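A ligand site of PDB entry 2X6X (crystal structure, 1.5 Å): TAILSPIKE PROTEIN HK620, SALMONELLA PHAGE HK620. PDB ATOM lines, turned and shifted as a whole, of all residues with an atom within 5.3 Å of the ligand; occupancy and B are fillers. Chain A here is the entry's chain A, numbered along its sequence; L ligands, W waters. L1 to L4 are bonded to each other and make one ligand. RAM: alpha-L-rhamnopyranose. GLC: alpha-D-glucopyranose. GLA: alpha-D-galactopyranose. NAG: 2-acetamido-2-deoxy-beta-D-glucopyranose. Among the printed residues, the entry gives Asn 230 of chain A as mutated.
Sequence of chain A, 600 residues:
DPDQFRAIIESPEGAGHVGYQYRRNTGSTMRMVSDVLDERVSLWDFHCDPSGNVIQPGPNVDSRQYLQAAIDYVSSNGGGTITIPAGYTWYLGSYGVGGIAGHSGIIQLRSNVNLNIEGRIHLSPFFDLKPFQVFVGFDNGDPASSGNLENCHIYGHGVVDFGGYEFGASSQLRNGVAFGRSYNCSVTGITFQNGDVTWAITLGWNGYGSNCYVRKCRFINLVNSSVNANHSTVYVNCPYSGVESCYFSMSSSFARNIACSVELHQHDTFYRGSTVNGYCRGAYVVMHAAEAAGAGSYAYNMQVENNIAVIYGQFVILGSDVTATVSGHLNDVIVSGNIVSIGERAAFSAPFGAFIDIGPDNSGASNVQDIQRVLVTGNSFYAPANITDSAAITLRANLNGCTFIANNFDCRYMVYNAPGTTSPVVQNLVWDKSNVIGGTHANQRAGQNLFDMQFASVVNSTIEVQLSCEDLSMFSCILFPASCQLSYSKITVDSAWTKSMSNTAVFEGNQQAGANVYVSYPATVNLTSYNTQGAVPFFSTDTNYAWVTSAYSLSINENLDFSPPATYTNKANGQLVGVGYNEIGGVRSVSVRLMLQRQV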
ATOM      1  N   GLY A 102     -19.533  20.365  37.648  1.00  0.00           N
ATOM      2  CA  GLY A 102     -20.978  20.218  37.468  1.00  0.00           C
ATOM      3  C   GLY A 102     -21.385  19.656  36.106  1.00  0.00           C
ATOM      4  O   GLY A 102     -22.558  19.288  35.913  1.00  0.00           O
ATOM      5  N   HIS A 103     -20.431  19.570  35.188  1.00  0.00           N
ATOM      6  CA  HIS A 103     -20.661  19.047  33.850  1.00  0.00           C
ATOM      7  C   HIS A 103     -19.926  17.724  33.659  1.00  0.00           C
ATOM      8  O   HIS A 103     -19.760  17.271  32.527  1.00  0.00           O
ATOM      9  CB  HIS A 103     -20.181  20.056  32.788  1.00  0.00           C
ATOM     10  CG  HIS A 103     -20.773  21.421  32.939  1.00  0.00           C
ATOM     11  ND1 HIS A 103     -21.970  21.785  32.363  1.00  0.00           N
ATOM     12  CD2 HIS A 103     -20.327  22.522  33.588  1.00  0.00           C
ATOM     13  CE1 HIS A 103     -22.230  23.052  32.650  1.00  0.00           C
ATOM     14  NE2 HIS A 103     -21.256  23.517  33.400  1.00  0.00           N
ATOM     15  N   GLN A 133     -17.695  14.677  30.315  1.00  0.00           N
ATOM     16  CA  GLN A 133     -17.647  15.574  29.167  1.00  0.00           C
ATOM     17  C   GLN A 133     -16.209  15.976  29.022  1.00  0.00           C
ATOM     18  O   GLN A 133     -15.657  16.636  29.900  1.00  0.00           O
ATOM     19  CB  GLN A 133     -18.557  16.790  29.362  1.00  0.00           C
ATOM     20  CG  GLN A 133     -20.025  16.374  29.480  1.00  0.00           C
ATOM     21  CD  GLN A 133     -20.992  17.539  29.296  1.00  0.00           C
ATOM     22  OE1 GLN A 133     -20.967  18.264  28.281  1.00  0.00           O
ATOM     23  NE2 GLN A 133     -21.879  17.724  30.288  1.00  0.00           N
ATOM     24  N   PHE A 138     -17.762  25.830  29.475  1.00  0.00           N
ATOM     25  CA  PHE A 138     -18.408  26.544  30.576  1.00  0.00           C
ATOM     26  C   PHE A 138     -17.373  26.757  31.679  1.00  0.00           C
ATOM     27  O   PHE A 138     -16.464  25.949  31.835  1.00  0.00           O
ATOM     28  CB  PHE A 138     -19.548  25.715  31.164  1.00  0.00           C
ATOM     29  CG  PHE A 138     -20.709  25.459  30.223  1.00  0.00           C
ATOM     30  CD1 PHE A 138     -21.619  26.467  29.932  1.00  0.00           C
ATOM     31  CD2 PHE A 138     -20.936  24.186  29.700  1.00  0.00           C
ATOM     32  CE1 PHE A 138     -22.715  26.213  29.104  1.00  0.00           C
ATOM     33  CE2 PHE A 138     -22.016  23.945  28.904  1.00  0.00           C
ATOM     34  CZ  PHE A 138     -22.912  24.963  28.607  1.00  0.00           C
ATOM     35  N   PRO A 143     -24.837  26.644  33.870  1.00  0.00           N
ATOM     36  CA  PRO A 143     -24.560  27.350  32.616  1.00  0.00           C
ATOM     37  C   PRO A 143     -25.105  28.781  32.561  1.00  0.00           C
ATOM     38  O   PRO A 143     -24.507  29.635  31.900  1.00  0.00           O
ATOM     39  CB  PRO A 143     -25.202  26.452  31.557  1.00  0.00           C
ATOM     40  CG  PRO A 143     -26.094  25.530  32.248  1.00  0.00           C
ATOM     41  CD  PRO A 143     -25.600  25.407  33.673  1.00  0.00           C
ATOM     42  N   LEU A 173     -24.941  11.509  31.314  1.00  0.00           N
ATOM     43  CA  LEU A 173     -24.642  12.227  30.081  1.00  0.00           C
ATOM     44  C   LEU A 173     -23.158  12.097  29.777  1.00  0.00           C
ATOM     45  O   LEU A 173     -22.323  12.119  30.706  1.00  0.00           O
ATOM     46  CB  LEU A 173     -25.001  13.699  30.203  1.00  0.00           C
ATOM     47  CG  LEU A 173     -26.462  14.068  30.472  1.00  0.00           C
ATOM     48  CD1 LEU A 173     -26.566  15.564  30.795  1.00  0.00           C
ATOM     49  CD2 LEU A 173     -27.377  13.694  29.317  1.00  0.00           C
ATOM     50  N   THR A 198     -23.689  10.628  24.650  1.00  0.00           N
ATOM     51  CA  THR A 198     -24.929  11.363  24.358  1.00  0.00           C
ATOM     52  C   THR A 198     -24.758  12.258  23.127  1.00  0.00           C
ATOM     53  O   THR A 198     -25.629  12.321  22.276  1.00  0.00           O
ATOM     54  CB  THR A 198     -25.345  12.252  25.536  1.00  0.00           C
ATOM     55  OG1 THR A 198     -25.338  11.505  26.773  1.00  0.00           O
ATOM     56  CG2 THR A 198     -26.732  12.826  25.311  1.00  0.00           C
ATOM     57  N   TRP A 199     -23.624  12.959  23.087  1.00  0.00           N
ATOM     58  CA  TRP A 199     -23.213  13.830  21.962  1.00  0.00           C
ATOM     59  C   TRP A 199     -21.699  13.652  21.801  1.00  0.00           C
ATOM     60  O   TRP A 199     -21.016  13.271  22.775  1.00  0.00           O
ATOM     61  CB  TRP A 199     -23.486  15.307  22.242  1.00  0.00           C
ATOM     62  CG  TRP A 199     -24.819  15.629  22.877  1.00  0.00           C
ATOM     63  CD1 TRP A 199     -26.018  15.738  22.257  1.00  0.00           C
ATOM     64  CD2 TRP A 199     -25.060  15.918  24.262  1.00  0.00           C
ATOM     65  NE1 TRP A 199     -26.994  16.073  23.159  1.00  0.00           N
ATOM     66  CE2 TRP A 199     -26.433  16.170  24.403  1.00  0.00           C
ATOM     67  CE3 TRP A 199     -24.243  15.945  25.397  1.00  0.00           C
ATOM     68  CZ2 TRP A 199     -27.012  16.474  25.632  1.00  0.00           C
ATOM     69  CZ3 TRP A 199     -24.808  16.240  26.622  1.00  0.00           C
ATOM     70  CH2 TRP A 199     -26.190  16.509  26.734  1.00  0.00           C
ATOM     71  N   THR A 202     -21.188  19.618  21.353  1.00  0.00           N
ATOM     72  CA  THR A 202     -22.291  20.552  21.484  1.00  0.00           C
ATOM     73  C   THR A 202     -21.746  21.980  21.272  1.00  0.00           C
ATOM     74  O   THR A 202     -20.622  22.306  21.713  1.00  0.00           O
ATOM     75  CB  THR A 202     -23.044  20.417  22.827  1.00  0.00           C
ATOM     76  OG1 THR A 202     -22.198  20.763  23.924  1.00  0.00           O
ATOM     77  CG2 THR A 202     -23.553  18.988  23.014  1.00  0.00           C
ATOM     78  N   GLY A 204     -22.743  26.079  21.662  1.00  0.00           N
ATOM     79  CA  GLY A 204     -23.652  27.029  22.303  1.00  0.00           C
ATOM     80  C   GLY A 204     -24.399  26.482  23.503  1.00  0.00           C
ATOM     81  O   GLY A 204     -24.281  25.309  23.860  1.00  0.00           O
ATOM     82  N   TRP A 205     -25.210  27.341  24.100  1.00  0.00           N
ATOM     83  CA  TRP A 205     -26.051  26.965  25.217  1.00  0.00           C
ATOM     84  C   TRP A 205     -27.310  27.830  25.179  1.00  0.00           C
ATOM     85  O   TRP A 205     -27.225  29.031  25.358  1.00  0.00           O
ATOM     86  CB  TRP A 205     -25.343  27.137  26.580  1.00  0.00           C
ATOM     87  CG  TRP A 205     -26.295  26.855  27.678  1.00  0.00           C
ATOM     88  CD1 TRP A 205     -26.789  25.631  28.042  1.00  0.00           C
ATOM     89  CD2 TRP A 205     -26.962  27.808  28.504  1.00  0.00           C
ATOM     90  NE1 TRP A 205     -27.684  25.767  29.056  1.00  0.00           N
ATOM     91  CE2 TRP A 205     -27.821  27.090  29.360  1.00  0.00           C
ATOM     92  CE3 TRP A 205     -26.905  29.193  28.602  1.00  0.00           C
ATOM     93  CZ2 TRP A 205     -28.608  27.727  30.311  1.00  0.00           C
ATOM     94  CZ3 TRP A 205     -27.701  29.829  29.548  1.00  0.00           C
ATOM     95  CH2 TRP A 205     -28.532  29.091  30.397  1.00  0.00           C
ATOM     96  N   ASN A 206     -28.453  27.203  24.881  1.00  0.00           N
ATOM     97  CA  ASN A 206     -29.767  27.867  24.871  1.00  0.00           C
ATOM     98  C   ASN A 206     -29.753  29.185  24.134  1.00  0.00           C
ATOM     99  O   ASN A 206     -30.253  30.196  24.592  1.00  0.00           O
ATOM    100  CB  ASN A 206     -30.303  27.998  26.302  1.00  0.00           C
ATOM    101  CG  ASN A 206     -30.632  26.648  26.909  1.00  0.00           C
ATOM    102  OD1 ASN A 206     -30.440  25.611  26.265  1.00  0.00           O
ATOM    103  ND2 ASN A 206     -31.101  26.656  28.144  1.00  0.00           N
ATOM    104  N   ASN A 230     -30.239   8.140  24.504  1.00  0.00           N
ATOM    105  CA  ASN A 230     -30.409   9.018  23.343  1.00  0.00           C
ATOM    106  C   ASN A 230     -29.057   9.502  22.876  1.00  0.00           C
ATOM    107  O   ASN A 230     -28.136   9.679  23.683  1.00  0.00           O
ATOM    108  CB  ASN A 230     -31.286  10.210  23.738  1.00  0.00           C
ATOM    109  CG  ASN A 230     -31.597  11.131  22.557  1.00  0.00           C
ATOM    110  OD1 ASN A 230     -31.852  10.685  21.450  1.00  0.00           O
ATOM    111  ND2 ASN A 230     -31.576  12.437  22.821  1.00  0.00           N
ATOM    112  N   TYR A 235     -24.864  18.803  18.385  1.00  0.00           N
ATOM    113  CA  TYR A 235     -26.039  19.557  18.829  1.00  0.00           C
ATOM    114  C   TYR A 235     -25.707  21.044  18.692  1.00  0.00           C
ATOM    115  O   TYR A 235     -24.811  21.562  19.387  1.00  0.00           O
ATOM    116  CB  TYR A 235     -26.387  19.205  20.274  1.00  0.00           C
ATOM    117  CG  TYR A 235     -27.771  19.553  20.766  1.00  0.00           C
ATOM    118  CD1 TYR A 235     -28.118  20.860  21.084  1.00  0.00           C
ATOM    119  CD2 TYR A 235     -28.731  18.561  20.972  1.00  0.00           C
ATOM    120  CE1 TYR A 235     -29.380  21.172  21.565  1.00  0.00           C
ATOM    121  CE2 TYR A 235     -29.989  18.864  21.466  1.00  0.00           C
ATOM    122  CZ  TYR A 235     -30.313  20.170  21.762  1.00  0.00           C
ATOM    123  OH  TYR A 235     -31.575  20.464  22.266  1.00  0.00           O
ATOM    124  N   ASN A 237     -26.662  24.619  19.293  1.00  0.00           N
ATOM    125  CA  ASN A 237     -27.542  25.397  20.164  1.00  0.00           C
ATOM    126  C   ASN A 237     -27.140  26.884  20.257  1.00  0.00           C
ATOM    127  O   ASN A 237     -27.392  27.563  21.240  1.00  0.00           O
ATOM    128  CB  ASN A 237     -27.637  24.758  21.556  1.00  0.00           C
ATOM    129  CG  ASN A 237     -28.963  25.023  22.232  1.00  0.00           C
ATOM    130  OD1 ASN A 237     -29.860  25.618  21.653  1.00  0.00           O
ATOM    131  ND2 ASN A 237     -29.101  24.561  23.466  1.00  0.00           N
ATOM    132  N   GLU A 263     -28.465  17.985  15.468  1.00  0.00           N
ATOM    133  CA  GLU A 263     -29.669  18.749  15.794  1.00  0.00           C
ATOM    134  C   GLU A 263     -29.371  20.228  15.571  1.00  0.00           C
ATOM    135  O   GLU A 263     -28.335  20.752  16.022  1.00  0.00           O
ATOM    136  CB  GLU A 263     -30.169  18.529  17.207  1.00  0.00           C
ATOM    137  CG  GLU A 263     -30.318  17.076  17.575  1.00  0.00           C
ATOM    138  CD  GLU A 263     -31.248  16.854  18.772  1.00  0.00           C
ATOM    139  OE1 GLU A 263     -32.196  17.649  18.994  1.00  0.00           O
ATOM    140  OE2 GLU A 263     -31.041  15.853  19.495  1.00  0.00           O
ATOM    141  N   HIS A 288     -37.099  24.630  20.466  1.00  0.00           N
ATOM    142  CA  HIS A 288     -37.532  24.328  21.830  1.00  0.00           C
ATOM    143  C   HIS A 288     -37.665  25.645  22.578  1.00  0.00           C
ATOM    144  O   HIS A 288     -36.679  26.337  22.755  1.00  0.00           O
ATOM    145  CB  HIS A 288     -36.486  23.489  22.569  1.00  0.00           C
ATOM    146  CG  HIS A 288     -36.427  22.046  22.174  1.00  0.00           C
ATOM    147  ND1 HIS A 288     -37.544  21.251  22.024  1.00  0.00           N
ATOM    148  CD2 HIS A 288     -35.363  21.236  21.969  1.00  0.00           C
ATOM    149  CE1 HIS A 288     -37.164  20.027  21.718  1.00  0.00           C
ATOM    150  NE2 HIS A 288     -35.846  19.991  21.671  1.00  0.00           N
ATOM    151  N   ALA A 290     -37.815  25.981  25.699  1.00  0.00           N
ATOM    152  CA  ALA A 290     -36.882  25.911  26.821  1.00  0.00           C
ATOM    153  C   ALA A 290     -35.456  26.378  26.474  1.00  0.00           C
ATOM    154  O   ALA A 290     -34.637  26.598  27.382  1.00  0.00           O
ATOM    155  CB  ALA A 290     -36.845  24.493  27.410  1.00  0.00           C
ATOM    156  N   GLU A 291     -35.156  26.519  25.173  1.00  0.00           N
ATOM    157  CA  GLU A 291     -33.842  26.952  24.700  1.00  0.00           C
ATOM    158  C   GLU A 291     -33.807  28.371  24.081  1.00  0.00           C
ATOM    159  O   GLU A 291     -32.829  28.750  23.457  1.00  0.00           O
ATOM    160  CB  GLU A 291     -33.299  25.912  23.712  1.00  0.00           C
ATOM    161  CG  GLU A 291     -33.142  24.528  24.305  1.00  0.00           C
ATOM    162  CD  GLU A 291     -32.662  23.523  23.281  1.00  0.00           C
ATOM    163  OE1 GLU A 291     -32.926  23.722  22.075  1.00  0.00           O
ATOM    164  OE2 GLU A 291     -32.046  22.533  23.676  1.00  0.00           O
ATOM    165  N   ASN A 362     -41.685  16.521  23.162  1.00  0.00           N
ATOM    166  CA  ASN A 362     -41.098  15.452  23.988  1.00  0.00           C
ATOM    167  C   ASN A 362     -42.122  14.719  24.859  1.00  0.00           C
ATOM    168  O   ASN A 362     -41.962  13.532  25.137  1.00  0.00           O
ATOM    169  CB  ASN A 362     -39.950  15.984  24.872  1.00  0.00           C
ATOM    170  CG  ASN A 362     -38.704  16.378  24.060  1.00  0.00           C
ATOM    171  OD1 ASN A 362     -38.590  16.030  22.882  1.00  0.00           O
ATOM    172  ND2 ASN A 362     -37.782  17.093  24.700  1.00  0.00           N
HETATM  173  C1  RAM L   1     -27.627  19.835  31.368  1.00  0.00           C
HETATM  174  C2  RAM L   1     -26.687  19.164  32.370  1.00  0.00           C
HETATM  175  C3  RAM L   1     -25.249  19.076  31.845  1.00  0.00           C
HETATM  176  C4  RAM L   1     -24.805  20.423  31.278  1.00  0.00           C
HETATM  177  C5  RAM L   1     -25.828  20.938  30.240  1.00  0.00           C
HETATM  178  C6  RAM L   1     -25.490  22.337  29.738  1.00  0.00           C
HETATM  179  O2  RAM L   1     -26.722  19.935  33.530  1.00  0.00           O
HETATM  180  O3  RAM L   1     -24.342  18.676  32.871  1.00  0.00           O
HETATM  181  O4  RAM L   1     -23.515  20.247  30.725  1.00  0.00           O
HETATM  182  O5  RAM L   1     -27.107  21.049  30.848  1.00  0.00           O
HETATM  183  C1  GLC L   2     -30.279  16.018  28.550  1.00  0.00           C
HETATM  184  C2  GLC L   2     -30.952  15.685  29.878  1.00  0.00           C
HETATM  185  C3  GLC L   2     -31.576  16.934  30.495  1.00  0.00           C
HETATM  186  C4  GLC L   2     -30.514  18.016  30.621  1.00  0.00           C
HETATM  187  C5  GLC L   2     -29.869  18.265  29.249  1.00  0.00           C
HETATM  188  C6  GLC L   2     -28.693  19.232  29.262  1.00  0.00           C
HETATM  189  O2  GLC L   2     -31.948  14.733  29.586  1.00  0.00           O
HETATM  190  O3  GLC L   2     -32.142  16.650  31.764  1.00  0.00           O
HETATM  191  O4  GLC L   2     -31.115  19.185  31.096  1.00  0.00           O
HETATM  192  O5  GLC L   2     -29.346  17.052  28.758  1.00  0.00           O
HETATM  193  O6  GLC L   2     -27.871  18.951  30.303  1.00  0.00           O
HETATM  194  C1  GLA L   3     -33.296  16.507  24.869  1.00  0.00           C
HETATM  195  C2  GLA L   3     -32.834  17.867  25.364  1.00  0.00           C
HETATM  196  C3  GLA L   3     -31.322  17.760  25.606  1.00  0.00           C
HETATM  197  C4  GLA L   3     -30.910  16.433  26.287  1.00  0.00           C
HETATM  198  C5  GLA L   3     -31.383  15.208  25.472  1.00  0.00           C
HETATM  199  C6  GLA L   3     -31.193  13.852  26.150  1.00  0.00           C
HETATM  200  O1  GLA L   3     -32.761  16.586  23.562  1.00  0.00           O
HETATM  201  O2  GLA L   3     -33.135  18.868  24.433  1.00  0.00           O
HETATM  202  O3  GLA L   3     -30.929  18.904  26.326  1.00  0.00           O
HETATM  203  O4  GLA L   3     -31.240  16.401  27.587  1.00  0.00           O
HETATM  204  O5  GLA L   3     -32.759  15.229  25.092  1.00  0.00           O
HETATM  205  O6  GLA L   3     -30.032  13.237  25.690  1.00  0.00           O
HETATM  206  C1  NAG L   4     -30.263  19.883  25.693  1.00  0.00           C
HETATM  207  C2  NAG L   4     -30.414  21.174  26.502  1.00  0.00           C
HETATM  208  C3  NAG L   4     -29.487  22.320  26.077  1.00  0.00           C
HETATM  209  C4  NAG L   4     -28.091  21.822  25.736  1.00  0.00           C
HETATM  210  C5  NAG L   4     -28.151  20.553  24.916  1.00  0.00           C
HETATM  211  C6  NAG L   4     -26.771  20.022  24.545  1.00  0.00           C
HETATM  212  C7  NAG L   4     -32.617  21.590  27.463  1.00  0.00           C
HETATM  213  C8  NAG L   4     -34.002  22.114  27.242  1.00  0.00           C
HETATM  214  N2  NAG L   4     -31.791  21.640  26.424  1.00  0.00           N
HETATM  215  O3  NAG L   4     -29.434  23.304  27.103  1.00  0.00           O
HETATM  216  O4  NAG L   4     -27.430  22.845  25.018  1.00  0.00           O
HETATM  217  O5  NAG L   4     -28.896  19.533  25.578  1.00  0.00           O
HETATM  218  O6  NAG L   4     -26.061  19.656  25.703  1.00  0.00           O
HETATM  219  O7  NAG L   4     -32.287  21.135  28.560  1.00  0.00           O
HETATM  220  O   HOH W   1     -22.411  20.542  28.302  1.00  0.00           O
HETATM  221  O   HOH W   2     -36.871  21.086  28.670  1.00  0.00           O
HETATM  222  O   HOH W   3     -30.973  12.736  31.341  1.00  0.00           O
HETATM  223  O   HOH W   4     -25.038  23.585  25.938  1.00  0.00           O
HETATM  224  O   HOH W   5     -23.081  16.009  33.082  1.00  0.00           O
HETATM  225  O   HOH W   6     -23.722  21.046  26.092  1.00  0.00           O
HETATM  226  O   HOH W   7     -28.930  23.072  29.968  1.00  0.00           O
HETATM  227  O   HOH W   8     -24.741  20.897  35.047  1.00  0.00           O
HETATM  228  O   HOH W   9     -28.740  12.886  22.746  1.00  0.00           O
HETATM  229  O   HOH W  10     -29.581  11.093  27.085  1.00  0.00           O
HETATM  230  O   HOH W  11     -33.873  17.494  21.151  1.00  0.00           O
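An oxygen (O3) of NAG L4 is in hydrogen-bond range of the side-chain amide oxygen of Asn 206 (2.7 Å).
An oxygen (O4) of RAM L1 sits at hydrogen-bond distance from a ring nitrogen (ND1) of His 103, at 2.7 Å.
An oxygen (O4) of NAG L4 sits at hydrogen-bond distance from the side-chain amide nitrogen (ND2) of Asn 237 (2.9 Å).
OE2 of Glu 291 lies within hydrogen-bond range of N2 of NAG L4 (2.9 Å).
NE2 of Gln 133 sits at hydrogen-bond distance from O4 of RAM L1 (3.0 Å).
The side-chain hydroxyl (OH) of Tyr 235 sits at hydrogen-bond distance from an oxygen (O2) of GLA L3, at 3.1 Å.
The side-chain amide nitrogen (ND2) of Asn 230 sits at hydrogen-bond distance from an oxygen (O6) of GLA L3 (3.4 Å).
The side-chain amide nitrogen of Asn 237 sits close to the backbone NH of Asn 206 (3.1 Å).
The side-chain amide nitrogen (NE2) of Gln 133 is in hydrogen-bond range of the backbone carbonyl oxygen (O) of His 103, at 3.1 Å.
The side-chain carboxylate (OE2) of Glu 291 is in hydrogen-bond range of the side-chain hydroxyl (OH) of Tyr 235, at 2.5 Å.
Residues that only touch the ligand: Gly 102, Phe 138, Leu 173, Thr 198, Trp 199, Thr 202, Trp 205 and Ala 290.
Hydrophobic or aromatic side chains that line the ligand: His 103, Phe 138, Leu 173, Trp 199, Trp 205, Tyr 235 and Ala 290.
The nearest printed residue that does not touch the ligand is His 288 (4.03 Å).
Water W4 lies within hydrogen-bond range of O4 of NAG L4 and O of Gly 204.
Water W1 bridges an oxygen (O4) of RAM L1 (2.7 Å) and the side-chain amide oxygen of Gln 133 (2.7 Å).
Water W6 lies within hydrogen-bond range of OG1 of Thr 202 (2.7 Å) and O6 of NAG L4 (2.7 Å).
Water W11 lies within hydrogen-bond range of the side-chain carboxylate of Glu 263 (2.7 Å), an oxygen (O1) of GLA L3 (2.8 Å) and a ring nitrogen (NE2) of His 288 (3.2 Å).
Water W7 lies within hydrogen-bond range of an oxygen (O5) of RAM L1 (2.9 Å) and the indole nitrogen (NE1) of Trp 205 (3.1 Å).
Water W9 lies within hydrogen-bond range of the side-chain amide nitrogen of Asn 230 (2.9 Å), the backbone carbonyl oxygen of Thr 198 (3.2 Å) and an oxygen (O6) of GLA L3 (3.2 Å).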
